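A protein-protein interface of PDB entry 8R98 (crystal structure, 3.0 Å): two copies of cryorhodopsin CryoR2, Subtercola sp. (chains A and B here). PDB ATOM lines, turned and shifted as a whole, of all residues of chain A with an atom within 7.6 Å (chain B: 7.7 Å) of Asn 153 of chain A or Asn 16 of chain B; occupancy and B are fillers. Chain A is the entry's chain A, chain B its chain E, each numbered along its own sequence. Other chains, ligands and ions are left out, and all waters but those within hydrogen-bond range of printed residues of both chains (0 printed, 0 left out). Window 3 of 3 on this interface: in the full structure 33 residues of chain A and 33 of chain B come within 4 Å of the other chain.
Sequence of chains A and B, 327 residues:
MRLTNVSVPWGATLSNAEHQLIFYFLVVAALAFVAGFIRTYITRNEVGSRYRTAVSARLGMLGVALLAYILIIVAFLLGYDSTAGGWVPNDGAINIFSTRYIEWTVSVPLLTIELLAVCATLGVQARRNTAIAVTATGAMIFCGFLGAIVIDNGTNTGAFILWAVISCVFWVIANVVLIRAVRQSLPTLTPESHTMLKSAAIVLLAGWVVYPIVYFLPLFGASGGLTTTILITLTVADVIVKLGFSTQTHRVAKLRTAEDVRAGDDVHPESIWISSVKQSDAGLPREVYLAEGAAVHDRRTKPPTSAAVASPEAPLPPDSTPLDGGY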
ATOM      1  N   VAL A   6       7.590 -43.077 -14.081  1.00  0.00           N
ATOM      2  CA  VAL A   6       8.353 -41.806 -13.883  1.00  0.00           C
ATOM      3  C   VAL A   6       8.366 -41.481 -12.386  1.00  0.00           C
ATOM      4  O   VAL A   6       7.273 -41.354 -11.804  1.00  0.00           O
ATOM      5  CB  VAL A   6       7.776 -40.624 -14.686  1.00  0.00           C
ATOM      6  CG1 VAL A   6       8.614 -39.370 -14.495  1.00  0.00           C
ATOM      7  CG2 VAL A   6       7.624 -40.950 -16.161  1.00  0.00           C
ATOM      8  N   VAL A   8       9.833 -38.542 -10.119  1.00  0.00           N
ATOM      9  CA  VAL A   8      10.414 -37.163 -10.070  1.00  0.00           C
ATOM     10  C   VAL A   8      11.637 -37.169  -9.155  1.00  0.00           C
ATOM     11  O   VAL A   8      11.574 -37.646  -8.025  1.00  0.00           O
ATOM     12  CB  VAL A   8       9.385 -36.102  -9.624  1.00  0.00           C
ATOM     13  CG1 VAL A   8       8.215 -36.008 -10.589  1.00  0.00           C
ATOM     14  CG2 VAL A   8       8.884 -36.345  -8.210  1.00  0.00           C
ATOM     15  N   TRP A  10      13.188 -34.638  -7.691  1.00  0.00           N
ATOM     16  CA  TRP A  10      13.069 -33.592  -6.638  1.00  0.00           C
ATOM     17  C   TRP A  10      12.217 -34.110  -5.475  1.00  0.00           C
ATOM     18  O   TRP A  10      11.920 -33.309  -4.560  1.00  0.00           O
ATOM     19  CB  TRP A  10      12.504 -32.286  -7.216  1.00  0.00           C
ATOM     20  CG  TRP A  10      11.210 -32.437  -7.956  1.00  0.00           C
ATOM     21  CD1 TRP A  10       9.958 -32.551  -7.422  1.00  0.00           C
ATOM     22  CD2 TRP A  10      11.041 -32.487  -9.382  1.00  0.00           C
ATOM     23  NE1 TRP A  10       9.025 -32.674  -8.417  1.00  0.00           N
ATOM     24  CE2 TRP A  10       9.658 -32.628  -9.630  1.00  0.00           C
ATOM     25  CE3 TRP A  10      11.920 -32.429 -10.470  1.00  0.00           C
ATOM     26  CZ2 TRP A  10       9.141 -32.715 -10.921  1.00  0.00           C
ATOM     27  CZ3 TRP A  10      11.405 -32.514 -11.746  1.00  0.00           C
ATOM     28  CH2 TRP A  10      10.034 -32.654 -11.967  1.00  0.00           C
ATOM     29  N   ASP A  91       9.053 -27.301  -1.837  1.00  0.00           N
ATOM     30  CA  ASP A  91       8.279 -26.919  -3.049  1.00  0.00           C
ATOM     31  C   ASP A  91       9.226 -26.371  -4.123  1.00  0.00           C
ATOM     32  O   ASP A  91       8.891 -26.489  -5.313  1.00  0.00           O
ATOM     33  CB  ASP A  91       7.220 -25.859  -2.732  1.00  0.00           C
ATOM     34  CG  ASP A  91       6.316 -26.208  -1.564  1.00  0.00           C
ATOM     35  OD1 ASP A  91       6.582 -27.230  -0.903  1.00  0.00           O
ATOM     36  OD2 ASP A  91       5.355 -25.450  -1.327  1.00  0.00           O
ATOM     37  N   ILE A  94      12.093 -28.490  -7.233  1.00  0.00           N
ATOM     38  CA  ILE A  94      11.808 -28.653  -8.691  1.00  0.00           C
ATOM     39  C   ILE A  94      12.540 -27.560  -9.479  1.00  0.00           C
ATOM     40  O   ILE A  94      12.979 -27.848 -10.613  1.00  0.00           O
ATOM     41  CB  ILE A  94      10.288 -28.630  -8.956  1.00  0.00           C
ATOM     42  CG1 ILE A  94       9.959 -28.936 -10.418  1.00  0.00           C
ATOM     43  CG2 ILE A  94       9.678 -27.304  -8.525  1.00  0.00           C
ATOM     44  CD1 ILE A  94       8.475 -28.996 -10.715  1.00  0.00           C
ATOM     45  N   LEU A 146       8.472 -29.165 -21.031  1.00  0.00           N
ATOM     46  CA  LEU A 146       7.005 -29.405 -20.970  1.00  0.00           C
ATOM     47  C   LEU A 146       6.757 -30.799 -20.399  1.00  0.00           C
ATOM     48  O   LEU A 146       5.992 -30.904 -19.428  1.00  0.00           O
ATOM     49  CB  LEU A 146       6.379 -29.273 -22.361  1.00  0.00           C
ATOM     50  CG  LEU A 146       6.522 -27.902 -23.013  1.00  0.00           C
ATOM     51  CD1 LEU A 146       5.888 -27.886 -24.393  1.00  0.00           C
ATOM     52  CD2 LEU A 146       5.914 -26.824 -22.128  1.00  0.00           C
ATOM     53  N   GLY A 147       7.395 -31.821 -20.972  1.00  0.00           N
ATOM     54  CA  GLY A 147       7.182 -33.227 -20.582  1.00  0.00           C
ATOM     55  C   GLY A 147       7.703 -33.528 -19.187  1.00  0.00           C
ATOM     56  O   GLY A 147       6.958 -34.147 -18.399  1.00  0.00           O
ATOM     57  N   ALA A 148       8.932 -33.107 -18.883  1.00  0.00           N
ATOM     58  CA  ALA A 148       9.625 -33.433 -17.616  1.00  0.00           C
ATOM     59  C   ALA A 148       9.044 -32.641 -16.440  1.00  0.00           C
ATOM     60  O   ALA A 148       8.913 -33.238 -15.354  1.00  0.00           O
ATOM     61  CB  ALA A 148      11.106 -33.189 -17.755  1.00  0.00           C
ATOM     62  N   ILE A 149       8.718 -31.359 -16.624  1.00  0.00           N
ATOM     63  CA  ILE A 149       8.330 -30.472 -15.485  1.00  0.00           C
ATOM     64  C   ILE A 149       6.898 -29.943 -15.641  1.00  0.00           C
ATOM     65  O   ILE A 149       6.096 -30.132 -14.701  1.00  0.00           O
ATOM     66  CB  ILE A 149       9.333 -29.310 -15.341  1.00  0.00           C
ATOM     67  CG1 ILE A 149      10.784 -29.758 -15.544  1.00  0.00           C
ATOM     68  CG2 ILE A 149       9.137 -28.626 -13.999  1.00  0.00           C
ATOM     69  CD1 ILE A 149      11.365 -30.535 -14.383  1.00  0.00           C
ATOM     70  N   VAL A 150       6.589 -29.295 -16.767  1.00  0.00           N
ATOM     71  CA  VAL A 150       5.300 -28.570 -16.978  1.00  0.00           C
ATOM     72  C   VAL A 150       4.104 -29.531 -16.931  1.00  0.00           C
ATOM     73  O   VAL A 150       3.132 -29.202 -16.225  1.00  0.00           O
ATOM     74  CB  VAL A 150       5.322 -27.765 -18.291  1.00  0.00           C
ATOM     75  CG1 VAL A 150       3.975 -27.122 -18.583  1.00  0.00           C
ATOM     76  CG2 VAL A 150       6.424 -26.720 -18.277  1.00  0.00           C
ATOM     77  N   ILE A 151       4.163 -30.669 -17.626  1.00  0.00           N
ATOM     78  CA  ILE A 151       2.990 -31.581 -17.776  1.00  0.00           C
ATOM     79  C   ILE A 151       2.804 -32.439 -16.522  1.00  0.00           C
ATOM     80  O   ILE A 151       3.714 -33.228 -16.193  1.00  0.00           O
ATOM     81  CB  ILE A 151       3.126 -32.451 -19.038  1.00  0.00           C
ATOM     82  CG1 ILE A 151       3.135 -31.585 -20.297  1.00  0.00           C
ATOM     83  CG2 ILE A 151       2.031 -33.504 -19.088  1.00  0.00           C
ATOM     84  CD1 ILE A 151       3.219 -32.378 -21.571  1.00  0.00           C
ATOM     85  N   ASP A 152       1.645 -32.295 -15.875  1.00  0.00           N
ATOM     86  CA  ASP A 152       1.233 -33.130 -14.718  1.00  0.00           C
ATOM     87  C   ASP A 152       2.360 -33.149 -13.683  1.00  0.00           C
ATOM     88  O   ASP A 152       2.586 -34.215 -13.058  1.00  0.00           O
ATOM     89  CB  ASP A 152       0.873 -34.539 -15.189  1.00  0.00           C
ATOM     90  CG  ASP A 152      -0.303 -34.558 -16.149  1.00  0.00           C
ATOM     91  OD1 ASP A 152      -0.902 -33.484 -16.365  1.00  0.00           O
ATOM     92  OD2 ASP A 152      -0.609 -35.645 -16.680  1.00  0.00           O
ATOM     93  N   ASN A 153       3.050 -32.017 -13.531  1.00  0.00           N
ATOM     94  CA  ASN A 153       4.106 -31.856 -12.502  1.00  0.00           C
ATOM     95  C   ASN A 153       5.178 -32.926 -12.733  1.00  0.00           C
ATOM     96  O   ASN A 153       5.803 -33.350 -11.744  1.00  0.00           O
ATOM     97  CB  ASN A 153       3.487 -31.938 -11.103  1.00  0.00           C
ATOM     98  CG  ASN A 153       2.306 -31.002 -10.949  1.00  0.00           C
ATOM     99  OD1 ASN A 153       2.107 -30.118 -11.779  1.00  0.00           O
ATOM    100  ND2 ASN A 153       1.509 -31.197  -9.908  1.00  0.00           N
ATOM    101  N   GLY A 154       5.368 -33.338 -13.993  1.00  0.00           N
ATOM    102  CA  GLY A 154       6.398 -34.312 -14.408  1.00  0.00           C
ATOM    103  C   GLY A 154       6.153 -35.696 -13.840  1.00  0.00           C
ATOM    104  O   GLY A 154       7.141 -36.440 -13.668  1.00  0.00           O
ATOM    105  N   THR A 155       4.893 -36.046 -13.576  1.00  0.00           N
ATOM    106  CA  THR A 155       4.531 -37.358 -12.972  1.00  0.00           C
ATOM    107  C   THR A 155       3.925 -38.289 -14.030  1.00  0.00           C
ATOM    108  O   THR A 155       3.543 -39.417 -13.663  1.00  0.00           O
ATOM    109  CB  THR A 155       3.593 -37.166 -11.774  1.00  0.00           C
ATOM    110  OG1 THR A 155       2.409 -36.531 -12.260  1.00  0.00           O
ATOM    111  CG2 THR A 155       4.237 -36.358 -10.668  1.00  0.00           C
ATOM    112  N   ASN A 156       3.856 -37.856 -15.289  1.00  0.00           N
ATOM    113  CA  ASN A 156       3.202 -38.632 -16.376  1.00  0.00           C
ATOM    114  C   ASN A 156       4.262 -39.293 -17.256  1.00  0.00           C
ATOM    115  O   ASN A 156       5.013 -38.557 -17.919  1.00  0.00           O
ATOM    116  CB  ASN A 156       2.293 -37.757 -17.240  1.00  0.00           C
ATOM    117  CG  ASN A 156       1.661 -38.515 -18.387  1.00  0.00           C
ATOM    118  OD1 ASN A 156       1.854 -39.718 -18.523  1.00  0.00           O
ATOM    119  ND2 ASN A 156       0.904 -37.821 -19.216  1.00  0.00           N
ATOM    120  N   LEU B  14      -2.772 -19.246  -9.902  1.00  0.00           N
ATOM    121  CA  LEU B  14      -2.005 -19.946 -10.969  1.00  0.00           C
ATOM    122  C   LEU B  14      -1.719 -21.399 -10.574  1.00  0.00           C
ATOM    123  O   LEU B  14      -1.447 -21.657  -9.381  1.00  0.00           O
ATOM    124  CB  LEU B  14      -0.697 -19.190 -11.217  1.00  0.00           C
ATOM    125  CG  LEU B  14      -0.842 -17.738 -11.665  1.00  0.00           C
ATOM    126  CD1 LEU B  14       0.523 -17.101 -11.862  1.00  0.00           C
ATOM    127  CD2 LEU B  14      -1.667 -17.630 -12.938  1.00  0.00           C
ATOM    128  N   SER B  15      -1.772 -22.304 -11.557  1.00  0.00           N
ATOM    129  CA  SER B  15      -1.426 -23.742 -11.409  1.00  0.00           C
ATOM    130  C   SER B  15       0.097 -23.871 -11.307  1.00  0.00           C
ATOM    131  O   SER B  15       0.795 -22.922 -11.721  1.00  0.00           O
ATOM    132  CB  SER B  15      -1.967 -24.561 -12.553  1.00  0.00           C
ATOM    133  OG  SER B  15      -1.282 -24.260 -13.759  1.00  0.00           O
ATOM    134  N   ASN B  16       0.590 -24.993 -10.775  1.00  0.00           N
ATOM    135  CA  ASN B  16       2.045 -25.269 -10.632  1.00  0.00           C
ATOM    136  C   ASN B  16       2.692 -25.205 -12.020  1.00  0.00           C
ATOM    137  O   ASN B  16       3.790 -24.624 -12.137  1.00  0.00           O
ATOM    138  CB  ASN B  16       2.309 -26.603  -9.932  1.00  0.00           C
ATOM    139  CG  ASN B  16       1.938 -26.571  -8.464  1.00  0.00           C
ATOM    140  OD1 ASN B  16       1.512 -25.540  -7.948  1.00  0.00           O
ATOM    141  ND2 ASN B  16       2.100 -27.692  -7.782  1.00  0.00           N
ATOM    142  N   ALA B  17       2.024 -25.775 -13.028  1.00  0.00           N
ATOM    143  CA  ALA B  17       2.466 -25.786 -14.442  1.00  0.00           C
ATOM    144  C   ALA B  17       2.596 -24.342 -14.941  1.00  0.00           C
ATOM    145  O   ALA B  17       3.674 -23.986 -15.451  1.00  0.00           O
ATOM    146  CB  ALA B  17       1.495 -26.575 -15.283  1.00  0.00           C
ATOM    147  N   GLU B  18       1.531 -23.549 -14.783  1.00  0.00           N
ATOM    148  CA  GLU B  18       1.469 -22.122 -15.199  1.00  0.00           C
ATOM    149  C   GLU B  18       2.619 -21.355 -14.534  1.00  0.00           C
ATOM    150  O   GLU B  18       3.377 -20.673 -15.260  1.00  0.00           O
ATOM    151  CB  GLU B  18       0.107 -21.524 -14.838  1.00  0.00           C
ATOM    152  CG  GLU B  18      -1.037 -22.077 -15.673  1.00  0.00           C
ATOM    153  CD  GLU B  18      -2.428 -21.639 -15.242  1.00  0.00           C
ATOM    154  OE1 GLU B  18      -3.398 -21.976 -15.951  1.00  0.00           O
ATOM    155  OE2 GLU B  18      -2.540 -20.967 -14.198  1.00  0.00           O
ATOM    156  N   HIS B  19       2.750 -21.486 -13.209  1.00  0.00           N
ATOM    157  CA  HIS B  19       3.788 -20.813 -12.381  1.00  0.00           C
ATOM    158  C   HIS B  19       5.177 -21.108 -12.957  1.00  0.00           C
ATOM    159  O   HIS B  19       6.002 -20.175 -13.023  1.00  0.00           O
ATOM    160  CB  HIS B  19       3.679 -21.256 -10.915  1.00  0.00           C
ATOM    161  CG  HIS B  19       4.506 -20.439  -9.978  1.00  0.00           C
ATOM    162  ND1 HIS B  19       5.799 -20.786  -9.631  1.00  0.00           N
ATOM    163  CD2 HIS B  19       4.230 -19.295  -9.317  1.00  0.00           C
ATOM    164  CE1 HIS B  19       6.283 -19.888  -8.797  1.00  0.00           C
ATOM    165  NE2 HIS B  19       5.340 -18.963  -8.588  1.00  0.00           N
ATOM    166  N   GLN B  20       5.414 -22.361 -13.359  1.00  0.00           N
ATOM    167  CA  GLN B  20       6.714 -22.841 -13.898  1.00  0.00           C
ATOM    168  C   GLN B  20       6.978 -22.164 -15.248  1.00  0.00           C
ATOM    169  O   GLN B  20       8.083 -21.615 -15.428  1.00  0.00           O
ATOM    170  CB  GLN B  20       6.695 -24.364 -14.045  1.00  0.00           C
ATOM    171  CG  GLN B  20       8.073 -25.004 -13.944  1.00  0.00           C
ATOM    172  CD  GLN B  20       8.568 -25.071 -12.520  1.00  0.00           C
ATOM    173  OE1 GLN B  20       7.804 -24.929 -11.567  1.00  0.00           O
ATOM    174  NE2 GLN B  20       9.860 -25.304 -12.361  1.00  0.00           N
ATOM    175  N   LEU B  21       5.993 -22.202 -16.152  1.00  0.00           N
ATOM    176  CA  LEU B  21       6.076 -21.615 -17.518  1.00  0.00           C
ATOM    177  C   LEU B  21       6.482 -20.140 -17.425  1.00  0.00           C
ATOM    178  O   LEU B  21       7.482 -19.762 -18.069  1.00  0.00           O
ATOM    179  CB  LEU B  21       4.725 -21.773 -18.222  1.00  0.00           C
ATOM    180  CG  LEU B  21       4.421 -23.171 -18.759  1.00  0.00           C
ATOM    181  CD1 LEU B  21       3.005 -23.246 -19.310  1.00  0.00           C
ATOM    182  CD2 LEU B  21       5.426 -23.576 -19.826  1.00  0.00           C
ATOM    183  N   ILE B  22       5.735 -19.345 -16.653  1.00  0.00           N
ATOM    184  CA  ILE B  22       5.980 -17.883 -16.472  1.00  0.00           C
ATOM    185  C   ILE B  22       7.444 -17.675 -16.067  1.00  0.00           C
ATOM    186  O   ILE B  22       8.126 -16.855 -16.714  1.00  0.00           O
ATOM    187  CB  ILE B  22       5.006 -17.279 -15.440  1.00  0.00           C
ATOM    188  CG1 ILE B  22       3.547 -17.540 -15.822  1.00  0.00           C
ATOM    189  CG2 ILE B  22       5.282 -15.795 -15.248  1.00  0.00           C
ATOM    190  CD1 ILE B  22       2.548 -17.051 -14.801  1.00  0.00           C
ATOM    191  N   PHE B  76       7.800 -11.763  -8.976  1.00  0.00           N
ATOM    192  CA  PHE B  76       7.090 -13.024  -9.316  1.00  0.00           C
ATOM    193  C   PHE B  76       7.284 -14.049  -8.195  1.00  0.00           C
ATOM    194  O   PHE B  76       6.314 -14.754  -7.844  1.00  0.00           O
ATOM    195  CB  PHE B  76       7.579 -13.575 -10.659  1.00  0.00           C
ATOM    196  CG  PHE B  76       7.028 -14.934 -11.014  1.00  0.00           C
ATOM    197  CD1 PHE B  76       7.773 -16.081 -10.789  1.00  0.00           C
ATOM    198  CD2 PHE B  76       5.761 -15.067 -11.561  1.00  0.00           C
ATOM    199  CE1 PHE B  76       7.265 -17.329 -11.112  1.00  0.00           C
ATOM    200  CE2 PHE B  76       5.254 -16.317 -11.881  1.00  0.00           C
ATOM    201  CZ  PHE B  76       6.004 -17.447 -11.650  1.00  0.00           C
ATOM    202  N   ASP B  81       2.180 -17.322  -3.389  1.00  0.00           N
ATOM    203  CA  ASP B  81       2.391 -18.283  -2.274  1.00  0.00           C
ATOM    204  C   ASP B  81       1.809 -19.636  -2.698  1.00  0.00           C
ATOM    205  O   ASP B  81       0.692 -19.643  -3.249  1.00  0.00           O
ATOM    206  CB  ASP B  81       1.760 -17.762  -0.982  1.00  0.00           C
ATOM    207  CG  ASP B  81       2.290 -16.402  -0.559  1.00  0.00           C
ATOM    208  OD1 ASP B  81       3.471 -16.124  -0.838  1.00  0.00           O
ATOM    209  OD2 ASP B  81       1.517 -15.631   0.047  1.00  0.00           O
ATOM    210  N   SER B  82       2.550 -20.725  -2.465  1.00  0.00           N
ATOM    211  CA  SER B  82       2.160 -22.111  -2.845  1.00  0.00           C
ATOM    212  C   SER B  82       1.173 -22.662  -1.814  1.00  0.00           C
ATOM    213  O   SER B  82       1.482 -22.601  -0.607  1.00  0.00           O
ATOM    214  CB  SER B  82       3.355 -23.013  -2.978  1.00  0.00           C
ATOM    215  OG  SER B  82       2.966 -24.287  -3.474  1.00  0.00           O
ATOM    216  N   THR B  83       0.034 -23.178  -2.284  1.00  0.00           N
ATOM    217  CA  THR B  83      -1.056 -23.732  -1.436  1.00  0.00           C
ATOM    218  C   THR B  83      -1.517 -25.074  -2.011  1.00  0.00           C
ATOM    219  O   THR B  83      -0.797 -25.632  -2.862  1.00  0.00           O
ATOM    220  CB  THR B  83      -2.237 -22.756  -1.327  1.00  0.00           C
ATOM    221  OG1 THR B  83      -2.791 -22.592  -2.633  1.00  0.00           O
ATOM    222  CG2 THR B  83      -1.843 -21.412  -0.752  1.00  0.00           C
ATOM    223  N   ALA B  84      -2.670 -25.565  -1.547  1.00  0.00           N
ATOM    224  CA  ALA B  84      -3.303 -26.823  -1.999  1.00  0.00           C
ATOM    225  C   ALA B  84      -4.017 -26.580  -3.334  1.00  0.00           C
ATOM    226  O   ALA B  84      -4.196 -27.552  -4.091  1.00  0.00           O
ATOM    227  CB  ALA B  84      -4.257 -27.326  -0.943  1.00  0.00           C
ATOM    228  N   GLY B  85      -4.394 -25.326  -3.607  1.00  0.00           N
ATOM    229  CA  GLY B  85      -5.130 -24.916  -4.820  1.00  0.00           C
ATOM    230  C   GLY B  85      -4.213 -24.391  -5.910  1.00  0.00           C
ATOM    231  O   GLY B  85      -4.736 -23.998  -6.971  1.00  0.00           O
ATOM    232  N   GLY B  86      -2.897 -24.400  -5.670  1.00  0.00           N
ATOM    233  CA  GLY B  86      -1.874 -23.916  -6.620  1.00  0.00           C
ATOM    234  C   GLY B  86      -1.036 -22.800  -6.018  1.00  0.00           C
ATOM    235  O   GLY B  86      -0.557 -22.978  -4.879  1.00  0.00           O
ATOM    236  N   TRP B  87      -0.882 -21.689  -6.749  1.00  0.00           N
ATOM    237  CA  TRP B  87      -0.142 -20.477  -6.303  1.00  0.00           C
ATOM    238  C   TRP B  87      -1.119 -19.308  -6.143  1.00  0.00           C
ATOM    239  O   TRP B  87      -1.546 -18.750  -7.175  1.00  0.00           O
ATOM    240  CB  TRP B  87       0.981 -20.140  -7.286  1.00  0.00           C
ATOM    241  CG  TRP B  87       2.064 -21.170  -7.330  1.00  0.00           C
ATOM    242  CD1 TRP B  87       2.070 -22.327  -8.054  1.00  0.00           C
ATOM    243  CD2 TRP B  87       3.315 -21.135  -6.621  1.00  0.00           C
ATOM    244  NE1 TRP B  87       3.236 -23.013  -7.845  1.00  0.00           N
ATOM    245  CE2 TRP B  87       4.020 -22.305  -6.971  1.00  0.00           C
ATOM    246  CE3 TRP B  87       3.907 -20.232  -5.729  1.00  0.00           C
ATOM    247  CZ2 TRP B  87       5.283 -22.593  -6.454  1.00  0.00           C
ATOM    248  CZ3 TRP B  87       5.157 -20.515  -5.224  1.00  0.00           C
ATOM    249  CH2 TRP B  87       5.832 -21.681  -5.582  1.00  0.00           C
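No position is printed for both chains. Of the 5 pairs that touch across the chains among the printed residues, none has its exchanged pair printed and touching as well.
Among the printed residues, merely in contact across the chains: Ile 149 of chain A with Gln 20 of chain B, Val 150 of chain A with Ala 17 of chain B, Val 150 of chain A with Leu 21 of chain B and Asn 153 of chain A with Asn 16 of chain B.
Printed residues of chain B that touch a printed residue of chain A: Asn 16, Ala 17, Gln 20, Leu 21 and Ser 82. Hydrophobic or aromatic side chains of chain B within 4 Å of the printed part of chain A: Ala 17 and Leu 21. Along chain B the printed residues that touch a printed residue of chain A span positions 16 to 82. Hydrophobic or aromatic side chains of chain A within 4 Å of the printed part of chain B: Ile 149 and Val 150. Along chain A the printed residues that touch a printed residue of chain B span positions 91 to 153.
Printed residues of chain B within 4 Å of Ile 149 of chain A: Gln 20 (3.8 Å). Of the printed residues of chain B, Asn 153 of chain A touches Asn 16. Of the printed residues of chain A, Asn 16 of chain B touches Asn 153. Glu 18 of chain B touches none of the printed residues of chain A. Printed residues of chain A within 4 Å of Ser 82 of chain B: Asp 91 (3.4 Å). The nearest residue of chain A that does not touch Asn 16 of chain B is Val 150 of chain A (5.8 Å). The nearest printed residue of chain A that does not touch Gln 20 of chain B is Ile 94 of chain A (4.1 Å).
OD2 of Asp 91 of chain A is in hydrogen-bond range of OG of Ser 82 of chain B (3.4 Å).
N of Gly 154 of chain A is in hydrogen-bond range of O of Ile 149 of chain A. The side-chain amide oxygen (OD1) of Asn 16 of chain B sits at hydrogen-bond distance from the indole nitrogen (NE1) of Trp 87 of chain B (3.1 Å).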
